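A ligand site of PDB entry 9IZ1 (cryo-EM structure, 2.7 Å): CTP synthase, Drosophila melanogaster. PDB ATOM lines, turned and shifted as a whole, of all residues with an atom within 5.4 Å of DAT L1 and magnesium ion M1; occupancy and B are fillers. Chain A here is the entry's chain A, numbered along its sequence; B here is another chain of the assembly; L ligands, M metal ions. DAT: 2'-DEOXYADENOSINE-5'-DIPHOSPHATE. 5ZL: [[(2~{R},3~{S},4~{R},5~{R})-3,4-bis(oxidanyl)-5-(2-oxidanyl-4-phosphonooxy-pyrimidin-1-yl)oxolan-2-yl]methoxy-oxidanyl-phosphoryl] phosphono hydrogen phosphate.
N of Gly 15 sits close to O3A of DAT L1, 3.2 Å away. N1 of DAT L1 is in hydrogen-bond range of N of Leu 246 (3.2 Å). The side-chain amino group (NZ) of Lys 16 is in salt-bridge range of an oxygen (O31) of 5ZL L2. The side-chain carboxylate (OD1) of Asp 312 sits at hydrogen-bond distance from an oxygen (O3') of DAT L1 (3.5 Å). The side-chain amino group (NZ) of Lys 16 is in salt-bridge range of an oxygen (O1B) of DAT L1, 3.1 Å away. The side-chain hydroxyl (OG) of Ser 12 lies within hydrogen-bond range of an oxygen (O10) of 5ZL L2 (3.0 Å). O3A of DAT L1 lies within hydrogen-bond range of N of Gly 17. O of His 244 is in hydrogen-bond range of N6 of DAT L1 (3.3 Å). The side-chain amino group (NZ) of Lys 38 sits at hydrogen-bond distance from an oxygen (O12) of 5ZL L2. O2B of DAT L1 lies close to O of Ser 12 (2.8 Å). N of Val 18 lies close to O1A of DAT L1 (3.4 Å). The backbone NH (N) of Lys 16 lies within hydrogen-bond range of an oxygen (O1B) of DAT L1.
OD2 of Asp 70 lies close to NZ of Lys 38 (2.6 Å). The backbone carbonyl oxygen (O) of Ile 243 sits at hydrogen-bond distance from the guanidinium group (NH1) of Arg 216 (2.9 Å). O of Gly 13 lies within hydrogen-bond range of OG1 of Thr 188 of chain B, at 2.8 Å. The side-chain carboxylate of Asp 245 lies within salt-bridge range of the guanidinium group of Arg 216 (3.1 Å). N of Ala 187 of chain B is in hydrogen-bond range of OD2 of Asp 245 (3.5 Å). The guanidinium group (NE) of Arg 216 is in hydrogen-bond range of the backbone carbonyl oxygen (O) of Val 14, at 3.0 Å.
Gly 13 touches DAT L1. N of Val 14 touches O1B of DAT L1 (3.9 Å). Arg 216 touches DAT L1 (NH2 to C5, 3.6 Å). CG2 of Ile 243 touches N6 of DAT L1 (3.3 Å). Asp 245 touches DAT L1 (CA to N1, 3.6 Å). Val 252 touches DAT L1. Ala 187 of chain B touches DAT L1. Hydrophobic or aromatic side chains that line DAT L1: Val 18, Ile 243, Val 252 and Ala 187 of chain B. Of the 23 residues printed, 17 come within 4 Å of DAT L1. The nearest printed residue that does not touch DAT L1 is Ile 249 (4.4 Å).
Merely in contact with magnesium ion M1: Gly 17. Three residues have an atom within 4 Å of magnesium ion M1: Gly 17, Asp 70 and Glu 145.
Magnesium ion M1 is bound by OD2 of Asp 70 (2.1 Å), O3B of DAT L1 (2.1 Å), O33 of 5ZL L2 (2.2 Å), OD1 of Asp 70 (2.2 Å) and OE2 of Glu 145 (2.6 Å).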
ATOM      1  N   SER A  12      12.474  -3.830  -9.302  1.00  0.00           N
ATOM      2  CA  SER A  12      13.193  -4.409 -10.430  1.00  0.00           C
ATOM      3  C   SER A  12      12.759  -3.825 -11.771  1.00  0.00           C
ATOM      4  O   SER A  12      13.340  -4.183 -12.792  1.00  0.00           O
ATOM      5  CB  SER A  12      13.017  -5.921 -10.447  1.00  0.00           C
ATOM      6  OG  SER A  12      11.741  -6.282 -10.935  1.00  0.00           O
ATOM      7  N   GLY A  13      11.759  -2.953 -11.778  1.00  0.00           N
ATOM      8  CA  GLY A  13      11.372  -2.274 -12.998  1.00  0.00           C
ATOM      9  C   GLY A  13      11.884  -0.844 -13.014  1.00  0.00           C
ATOM     10  O   GLY A  13      11.372   0.004 -13.744  1.00  0.00           O
ATOM     11  N   VAL A  14      12.900  -0.590 -12.195  1.00  0.00           N
ATOM     12  CA  VAL A  14      13.374   0.775 -11.991  1.00  0.00           C
ATOM     13  C   VAL A  14      13.994   1.334 -13.269  1.00  0.00           C
ATOM     14  O   VAL A  14      13.865   2.525 -13.562  1.00  0.00           O
ATOM     15  CB  VAL A  14      14.348   0.827 -10.798  1.00  0.00           C
ATOM     16  CG1 VAL A  14      15.513  -0.129 -11.008  1.00  0.00           C
ATOM     17  CG2 VAL A  14      14.835   2.244 -10.560  1.00  0.00           C
ATOM     18  N   GLY A  15      14.657   0.483 -14.053  1.00  0.00           N
ATOM     19  CA  GLY A  15      15.300   0.958 -15.259  1.00  0.00           C
ATOM     20  C   GLY A  15      16.776   0.644 -15.369  1.00  0.00           C
ATOM     21  O   GLY A  15      17.513   1.378 -16.031  1.00  0.00           O
ATOM     22  N   LYS A  16      17.216  -0.444 -14.729  1.00  0.00           N
ATOM     23  CA  LYS A  16      18.626  -0.829 -14.801  1.00  0.00           C
ATOM     24  C   LYS A  16      19.054  -1.125 -16.239  1.00  0.00           C
ATOM     25  O   LYS A  16      20.182  -0.795 -16.632  1.00  0.00           O
ATOM     26  CB  LYS A  16      18.890  -2.049 -13.940  1.00  0.00           C
ATOM     27  CG  LYS A  16      18.687  -1.837 -12.457  1.00  0.00           C
ATOM     28  CD  LYS A  16      19.078  -3.098 -11.715  1.00  0.00           C
ATOM     29  CE  LYS A  16      18.243  -4.280 -12.161  1.00  0.00           C
ATOM     30  NZ  LYS A  16      16.828  -4.140 -11.741  1.00  0.00           N
ATOM     31  N   GLY A  17      18.187  -1.770 -17.020  1.00  0.00           N
ATOM     32  CA  GLY A  17      18.555  -2.097 -18.388  1.00  0.00           C
ATOM     33  C   GLY A  17      18.804  -0.876 -19.240  1.00  0.00           C
ATOM     34  O   GLY A  17      19.764  -0.827 -20.002  1.00  0.00           O
ATOM     35  N   VAL A  18      17.936   0.135 -19.106  1.00  0.00           N
ATOM     36  CA  VAL A  18      18.110   1.364 -19.872  1.00  0.00           C
ATOM     37  C   VAL A  18      19.365   2.103 -19.414  1.00  0.00           C
ATOM     38  O   VAL A  18      20.107   2.669 -20.232  1.00  0.00           O
ATOM     39  CB  VAL A  18      16.855   2.250 -19.768  1.00  0.00           C
ATOM     40  CG1 VAL A  18      17.133   3.647 -20.269  1.00  0.00           C
ATOM     41  CG2 VAL A  18      15.718   1.621 -20.558  1.00  0.00           C
ATOM     42  N   LYS A  38      24.454  -9.817 -18.784  1.00  0.00           N
ATOM     43  CA  LYS A  38      23.230  -9.785 -17.996  1.00  0.00           C
ATOM     44  C   LYS A  38      23.254 -10.944 -17.015  1.00  0.00           C
ATOM     45  O   LYS A  38      23.434 -12.100 -17.411  1.00  0.00           O
ATOM     46  CB  LYS A  38      21.996  -9.853 -18.878  1.00  0.00           C
ATOM     47  CG  LYS A  38      20.698  -9.924 -18.105  1.00  0.00           C
ATOM     48  CD  LYS A  38      20.546  -8.737 -17.180  1.00  0.00           C
ATOM     49  CE  LYS A  38      19.478  -8.976 -16.133  1.00  0.00           C
ATOM     50  NZ  LYS A  38      18.151  -9.263 -16.757  1.00  0.00           N
ATOM     51  N   LEU A  69      14.991  -9.839 -22.554  1.00  0.00           N
ATOM     52  CA  LEU A  69      14.933  -8.669 -23.420  1.00  0.00           C
ATOM     53  C   LEU A  69      16.044  -7.676 -23.146  1.00  0.00           C
ATOM     54  O   LEU A  69      16.274  -6.783 -23.966  1.00  0.00           O
ATOM     55  CB  LEU A  69      13.565  -7.984 -23.293  1.00  0.00           C
ATOM     56  CG  LEU A  69      13.127  -7.386 -21.949  1.00  0.00           C
ATOM     57  CD1 LEU A  69      13.554  -5.945 -21.797  1.00  0.00           C
ATOM     58  CD2 LEU A  69      11.620  -7.511 -21.808  1.00  0.00           C
ATOM     59  N   ASP A  70      16.739  -7.810 -22.014  1.00  0.00           N
ATOM     60  CA  ASP A  70      17.887  -6.942 -21.738  1.00  0.00           C
ATOM     61  C   ASP A  70      18.984  -7.132 -22.775  1.00  0.00           C
ATOM     62  O   ASP A  70      19.643  -6.174 -23.186  1.00  0.00           O
ATOM     63  CB  ASP A  70      18.414  -7.200 -20.336  1.00  0.00           C
ATOM     64  CG  ASP A  70      17.499  -6.649 -19.251  1.00  0.00           C
ATOM     65  OD1 ASP A  70      16.844  -5.626 -19.500  1.00  0.00           O
ATOM     66  OD2 ASP A  70      17.442  -7.249 -18.159  1.00  0.00           O
ATOM     67  N   ASN A  73      17.955  -5.166 -25.697  1.00  0.00           N
ATOM     68  CA  ASN A  73      18.291  -3.753 -25.509  1.00  0.00           C
ATOM     69  C   ASN A  73      19.780  -3.508 -25.745  1.00  0.00           C
ATOM     70  O   ASN A  73      20.158  -2.491 -26.336  1.00  0.00           O
ATOM     71  CB  ASN A  73      17.903  -3.295 -24.104  1.00  0.00           C
ATOM     72  CG  ASN A  73      16.426  -3.474 -23.821  1.00  0.00           C
ATOM     73  OD1 ASN A  73      16.050  -4.212 -22.912  1.00  0.00           O
ATOM     74  ND2 ASN A  73      15.590  -2.797 -24.587  1.00  0.00           N
ATOM     75  N   TYR A  74      20.627  -4.425 -25.276  1.00  0.00           N
ATOM     76  CA  TYR A  74      22.059  -4.285 -25.495  1.00  0.00           C
ATOM     77  C   TYR A  74      22.386  -4.301 -26.983  1.00  0.00           C
ATOM     78  O   TYR A  74      23.149  -3.456 -27.469  1.00  0.00           O
ATOM     79  CB  TYR A  74      22.816  -5.418 -24.785  1.00  0.00           C
ATOM     80  CG  TYR A  74      22.593  -5.491 -23.298  1.00  0.00           C
ATOM     81  CD1 TYR A  74      22.205  -4.375 -22.564  1.00  0.00           C
ATOM     82  CD2 TYR A  74      22.765  -6.688 -22.611  1.00  0.00           C
ATOM     83  CE1 TYR A  74      21.990  -4.448 -21.206  1.00  0.00           C
ATOM     84  CE2 TYR A  74      22.557  -6.773 -21.254  1.00  0.00           C
ATOM     85  CZ  TYR A  74      22.173  -5.651 -20.553  1.00  0.00           C
ATOM     86  OH  TYR A  74      21.959  -5.731 -19.202  1.00  0.00           O
ATOM     87  N   GLU A 145      25.107  -6.091 -15.454  1.00  0.00           N
ATOM     88  CA  GLU A 145      23.850  -5.715 -14.832  1.00  0.00           C
ATOM     89  C   GLU A 145      23.373  -6.852 -13.955  1.00  0.00           C
ATOM     90  O   GLU A 145      23.262  -7.998 -14.411  1.00  0.00           O
ATOM     91  CB  GLU A 145      22.784  -5.385 -15.892  1.00  0.00           C
ATOM     92  CG  GLU A 145      21.437  -5.014 -15.301  1.00  0.00           C
ATOM     93  CD  GLU A 145      20.315  -5.122 -16.304  1.00  0.00           C
ATOM     94  OE1 GLU A 145      20.599  -5.170 -17.520  1.00  0.00           O
ATOM     95  OE2 GLU A 145      19.141  -5.175 -15.884  1.00  0.00           O
ATOM     96  N   ARG A 216      15.573   7.488  -9.695  1.00  0.00           N
ATOM     97  CA  ARG A 216      14.525   7.396 -10.710  1.00  0.00           C
ATOM     98  C   ARG A 216      13.211   7.865 -10.116  1.00  0.00           C
ATOM     99  O   ARG A 216      12.766   7.359  -9.078  1.00  0.00           O
ATOM    100  CB  ARG A 216      14.394   5.963 -11.234  1.00  0.00           C
ATOM    101  CG  ARG A 216      15.535   5.535 -12.139  1.00  0.00           C
ATOM    102  CD  ARG A 216      15.336   6.036 -13.564  1.00  0.00           C
ATOM    103  NE  ARG A 216      14.131   5.483 -14.180  1.00  0.00           N
ATOM    104  CZ  ARG A 216      12.998   6.144 -14.338  1.00  0.00           C
ATOM    105  NH1 ARG A 216      12.872   7.402 -13.942  1.00  0.00           N
ATOM    106  NH2 ARG A 216      11.963   5.534 -14.911  1.00  0.00           N
ATOM    107  N   ILE A 243      17.313  10.858 -12.948  1.00  0.00           N
ATOM    108  CA  ILE A 243      16.708  10.530 -14.232  1.00  0.00           C
ATOM    109  C   ILE A 243      15.210  10.378 -14.006  1.00  0.00           C
ATOM    110  O   ILE A 243      14.773   9.522 -13.225  1.00  0.00           O
ATOM    111  CB  ILE A 243      17.292   9.241 -14.833  1.00  0.00           C
ATOM    112  CG1 ILE A 243      18.816   9.305 -14.840  1.00  0.00           C
ATOM    113  CG2 ILE A 243      16.758   9.027 -16.242  1.00  0.00           C
ATOM    114  CD1 ILE A 243      19.393  10.252 -15.859  1.00  0.00           C
ATOM    115  N   HIS A 244      14.421  11.201 -14.689  1.00  0.00           N
ATOM    116  CA  HIS A 244      12.971  11.150 -14.576  1.00  0.00           C
ATOM    117  C   HIS A 244      12.379  10.478 -15.809  1.00  0.00           C
ATOM    118  O   HIS A 244      13.084  10.108 -16.750  1.00  0.00           O
ATOM    119  CB  HIS A 244      12.389  12.549 -14.358  1.00  0.00           C
ATOM    120  CG  HIS A 244      12.672  13.499 -15.474  1.00  0.00           C
ATOM    121  ND1 HIS A 244      13.805  14.283 -15.515  1.00  0.00           N
ATOM    122  CD2 HIS A 244      11.968  13.795 -16.586  1.00  0.00           C
ATOM    123  CE1 HIS A 244      13.791  15.022 -16.611  1.00  0.00           C
ATOM    124  NE2 HIS A 244      12.684  14.753 -17.279  1.00  0.00           N
ATOM    125  N   ASP A 245      11.053  10.327 -15.814  1.00  0.00           N
ATOM    126  CA  ASP A 245      10.371   9.709 -16.937  1.00  0.00           C
ATOM    127  C   ASP A 245      10.436  10.623 -18.147  1.00  0.00           C
ATOM    128  O   ASP A 245       9.978  11.766 -18.103  1.00  0.00           O
ATOM    129  CB  ASP A 245       8.921   9.401 -16.577  1.00  0.00           C
ATOM    130  CG  ASP A 245       8.789   8.232 -15.612  1.00  0.00           C
ATOM    131  OD1 ASP A 245       9.835   7.730 -15.150  1.00  0.00           O
ATOM    132  OD2 ASP A 245       7.656   7.820 -15.322  1.00  0.00           O
ATOM    133  N   LEU A 246      11.018  10.119 -19.233  1.00  0.00           N
ATOM    134  CA  LEU A 246      11.213  10.886 -20.456  1.00  0.00           C
ATOM    135  C   LEU A 246      10.284  10.390 -21.551  1.00  0.00           C
ATOM    136  O   LEU A 246       9.644   9.349 -21.441  1.00  0.00           O
ATOM    137  CB  LEU A 246      12.677  10.814 -20.900  1.00  0.00           C
ATOM    138  CG  LEU A 246      13.695  11.266 -19.854  1.00  0.00           C
ATOM    139  CD1 LEU A 246      15.053  10.636 -20.109  1.00  0.00           C
ATOM    140  CD2 LEU A 246      13.809  12.786 -19.849  1.00  0.00           C
ATOM    141  N   ILE A 249      13.385   6.536 -24.607  1.00  0.00           N
ATOM    142  CA  ILE A 249      14.637   6.098 -23.995  1.00  0.00           C
ATOM    143  C   ILE A 249      15.862   6.670 -24.684  1.00  0.00           C
ATOM    144  O   ILE A 249      16.973   6.527 -24.153  1.00  0.00           O
ATOM    145  CB  ILE A 249      14.734   4.561 -23.981  1.00  0.00           C
ATOM    146  CG1 ILE A 249      14.591   4.003 -25.396  1.00  0.00           C
ATOM    147  CG2 ILE A 249      13.679   3.970 -23.061  1.00  0.00           C
ATOM    148  CD1 ILE A 249      14.724   2.510 -25.482  1.00  0.00           C
ATOM    149  N   VAL A 252      17.734   9.270 -22.458  1.00  0.00           N
ATOM    150  CA  VAL A 252      18.504   8.875 -21.283  1.00  0.00           C
ATOM    151  C   VAL A 252      20.006   9.074 -21.471  1.00  0.00           C
ATOM    152  O   VAL A 252      20.654   9.621 -20.564  1.00  0.00           O
ATOM    153  CB  VAL A 252      18.142   7.432 -20.871  1.00  0.00           C
ATOM    154  CG1 VAL A 252      18.811   7.067 -19.562  1.00  0.00           C
ATOM    155  CG2 VAL A 252      16.631   7.291 -20.757  1.00  0.00           C
ATOM    156  N   ASP A 312       5.125  -4.520 -21.961  1.00  0.00           N
ATOM    157  CA  ASP A 312       6.478  -4.909 -22.319  1.00  0.00           C
ATOM    158  C   ASP A 312       6.571  -6.332 -22.864  1.00  0.00           C
ATOM    159  O   ASP A 312       7.674  -6.807 -23.139  1.00  0.00           O
ATOM    160  CB  ASP A 312       7.404  -4.764 -21.110  1.00  0.00           C
ATOM    161  CG  ASP A 312       7.811  -3.326 -20.856  1.00  0.00           C
ATOM    162  OD1 ASP A 312       8.039  -2.596 -21.839  1.00  0.00           O
ATOM    163  OD2 ASP A 312       7.890  -2.934 -19.678  1.00  0.00           O
ATOM    164  N   ALA B 187       6.352   4.601 -15.575  1.00  0.00           N
ATOM    165  CA  ALA B 187       7.120   3.927 -16.617  1.00  0.00           C
ATOM    166  C   ALA B 187       6.940   2.420 -16.540  1.00  0.00           C
ATOM    167  O   ALA B 187       6.758   1.749 -17.571  1.00  0.00           O
ATOM    168  CB  ALA B 187       8.599   4.294 -16.491  1.00  0.00           C
ATOM    169  N   THR B 188       6.979   1.861 -15.340  1.00  0.00           N
ATOM    170  CA  THR B 188       6.825   0.416 -15.167  1.00  0.00           C
ATOM    171  C   THR B 188       5.378  -0.005 -15.392  1.00  0.00           C
ATOM    172  O   THR B 188       5.103  -1.020 -16.037  1.00  0.00           O
ATOM    173  CB  THR B 188       7.319  -0.002 -13.790  1.00  0.00           C
ATOM    174  OG1 THR B 188       8.644   0.501 -13.586  1.00  0.00           O
ATOM    175  CG2 THR B 188       7.357  -1.514 -13.691  1.00  0.00           C
HETATM  176  PB  DAT L   1      14.985  -3.134 -15.477  1.00  0.00           P
HETATM  177  O1B DAT L   1      15.487  -2.706 -14.131  1.00  0.00           O
HETATM  178  O2B DAT L   1      13.548  -3.561 -15.495  1.00  0.00           O
HETATM  179  O3B DAT L   1      15.929  -3.984 -16.283  1.00  0.00           O
HETATM  180  PA  DAT L   1      14.223  -1.578 -17.717  1.00  0.00           P
HETATM  181  O1A DAT L   1      14.665  -0.243 -18.242  1.00  0.00           O
HETATM  182  O2A DAT L   1      14.414  -2.807 -18.567  1.00  0.00           O
HETATM  183  O3A DAT L   1      14.990  -1.771 -16.320  1.00  0.00           O
HETATM  184  O5' DAT L   1      12.680  -1.473 -17.313  1.00  0.00           O
HETATM  185  C5' DAT L   1      12.089  -0.203 -17.065  1.00  0.00           C
HETATM  186  C4' DAT L   1      11.060   0.116 -18.139  1.00  0.00           C
HETATM  187  O4' DAT L   1      10.752   1.503 -18.117  1.00  0.00           O
HETATM  188  C3' DAT L   1      11.574  -0.188 -19.520  1.00  0.00           C
HETATM  189  O3' DAT L   1      10.545  -0.775 -20.301  1.00  0.00           O
HETATM  190  C2' DAT L   1      11.982   1.137 -20.122  1.00  0.00           C
HETATM  191  C1' DAT L   1      11.302   2.180 -19.249  1.00  0.00           C
HETATM  192  N9  DAT L   1      12.284   3.198 -18.781  1.00  0.00           N
HETATM  193  C8  DAT L   1      13.470   2.946 -18.206  1.00  0.00           C
HETATM  194  N7  DAT L   1      14.106   4.090 -17.893  1.00  0.00           N
HETATM  195  C5  DAT L   1      13.315   5.108 -18.261  1.00  0.00           C
HETATM  196  C6  DAT L   1      13.386   6.585 -18.215  1.00  0.00           C
HETATM  197  N6  DAT L   1      14.457   7.212 -17.700  1.00  0.00           N
HETATM  198  N1  DAT L   1      12.339   7.276 -18.712  1.00  0.00           N
HETATM  199  C2  DAT L   1      11.269   6.659 -19.237  1.00  0.00           C
HETATM  200  N3  DAT L   1      11.137   5.329 -19.308  1.00  0.00           N
HETATM  201  C4  DAT L   1      12.111   4.514 -18.848  1.00  0.00           C
HETATM  202  C21 5ZL L   2      14.060 -12.666  -8.421  1.00  0.00           C
HETATM  203  C22 5ZL L   2      15.038 -11.903  -9.293  1.00  0.00           C
HETATM  204  C24 5ZL L   2      14.716 -12.426 -10.743  1.00  0.00           C
HETATM  205  C26 5ZL L   2      16.005 -11.715 -12.640  1.00  0.00           C
HETATM  206  C28 5ZL L   2      14.810  -9.309 -12.679  1.00  0.00           C
HETATM  207  C23 5ZL L   2      13.004 -12.943  -9.219  1.00  0.00           C
HETATM  208  C25 5ZL L   2      11.837 -12.111  -8.811  1.00  0.00           C
HETATM  209  C27 5ZL L   2      14.454 -10.251 -11.719  1.00  0.00           C
HETATM  210  C29 5ZL L   2      15.789  -9.620 -13.616  1.00  0.00           C
HETATM  211  N19 5ZL L   2      15.080 -11.427 -11.747  1.00  0.00           N
HETATM  212  N20 5ZL L   2      16.351 -10.839 -13.547  1.00  0.00           N
HETATM  213  O04 5ZL L   2      13.422 -12.617 -10.733  1.00  0.00           O
HETATM  214  O05 5ZL L   2      14.698 -13.945  -7.957  1.00  0.00           O
HETATM  215  O07 5ZL L   2      11.706 -11.007  -9.745  1.00  0.00           O
HETATM  216  O08 5ZL L   2      16.640 -13.018 -12.622  1.00  0.00           O
HETATM  217  O09 5ZL L   2      10.246  -9.780  -7.747  1.00  0.00           O
HETATM  218  O10 5ZL L   2      12.109  -8.525  -8.953  1.00  0.00           O
HETATM  219  O11 5ZL L   2      10.045  -8.999 -10.200  1.00  0.00           O
HETATM  220  O12 5ZL L   2      16.185  -8.693 -14.615  1.00  0.00           O
HETATM  221  O13 5ZL L   2       8.083  -8.434  -6.938  1.00  0.00           O
HETATM  222  O14 5ZL L   2       8.315 -10.973  -6.552  1.00  0.00           O
HETATM  223  O15 5ZL L   2       7.944 -10.163  -8.834  1.00  0.00           O
HETATM  224  O16 5ZL L   2       6.040  -7.015  -7.523  1.00  0.00           O
HETATM  225  O17 5ZL L   2       7.645  -7.482  -9.312  1.00  0.00           O
HETATM  226  O18 5ZL L   2       8.233  -5.925  -7.480  1.00  0.00           O
HETATM  227  O31 5ZL L   2      16.290  -6.618 -13.004  1.00  0.00           O
HETATM  228  O32 5ZL L   2      14.315  -6.900 -14.496  1.00  0.00           O
HETATM  229  O33 5ZL L   2      16.475  -6.250 -15.450  1.00  0.00           O
HETATM  230  P01 5ZL L   2      11.012  -9.533  -9.169  1.00  0.00           P
HETATM  231  P02 5ZL L   2       8.627  -9.858  -7.549  1.00  0.00           P
HETATM  232  P03 5ZL L   2       7.482  -7.192  -7.834  1.00  0.00           P
HETATM  233  P30 5ZL L   2      15.806  -7.072 -14.393  1.00  0.00           P
HETATM  234 MG    MG M   1      17.059  -5.379 -17.348  1.00  0.00          MG
HETATM  235 MG    MG M   2      13.224  -6.132 -15.989  1.00  0.00          MG
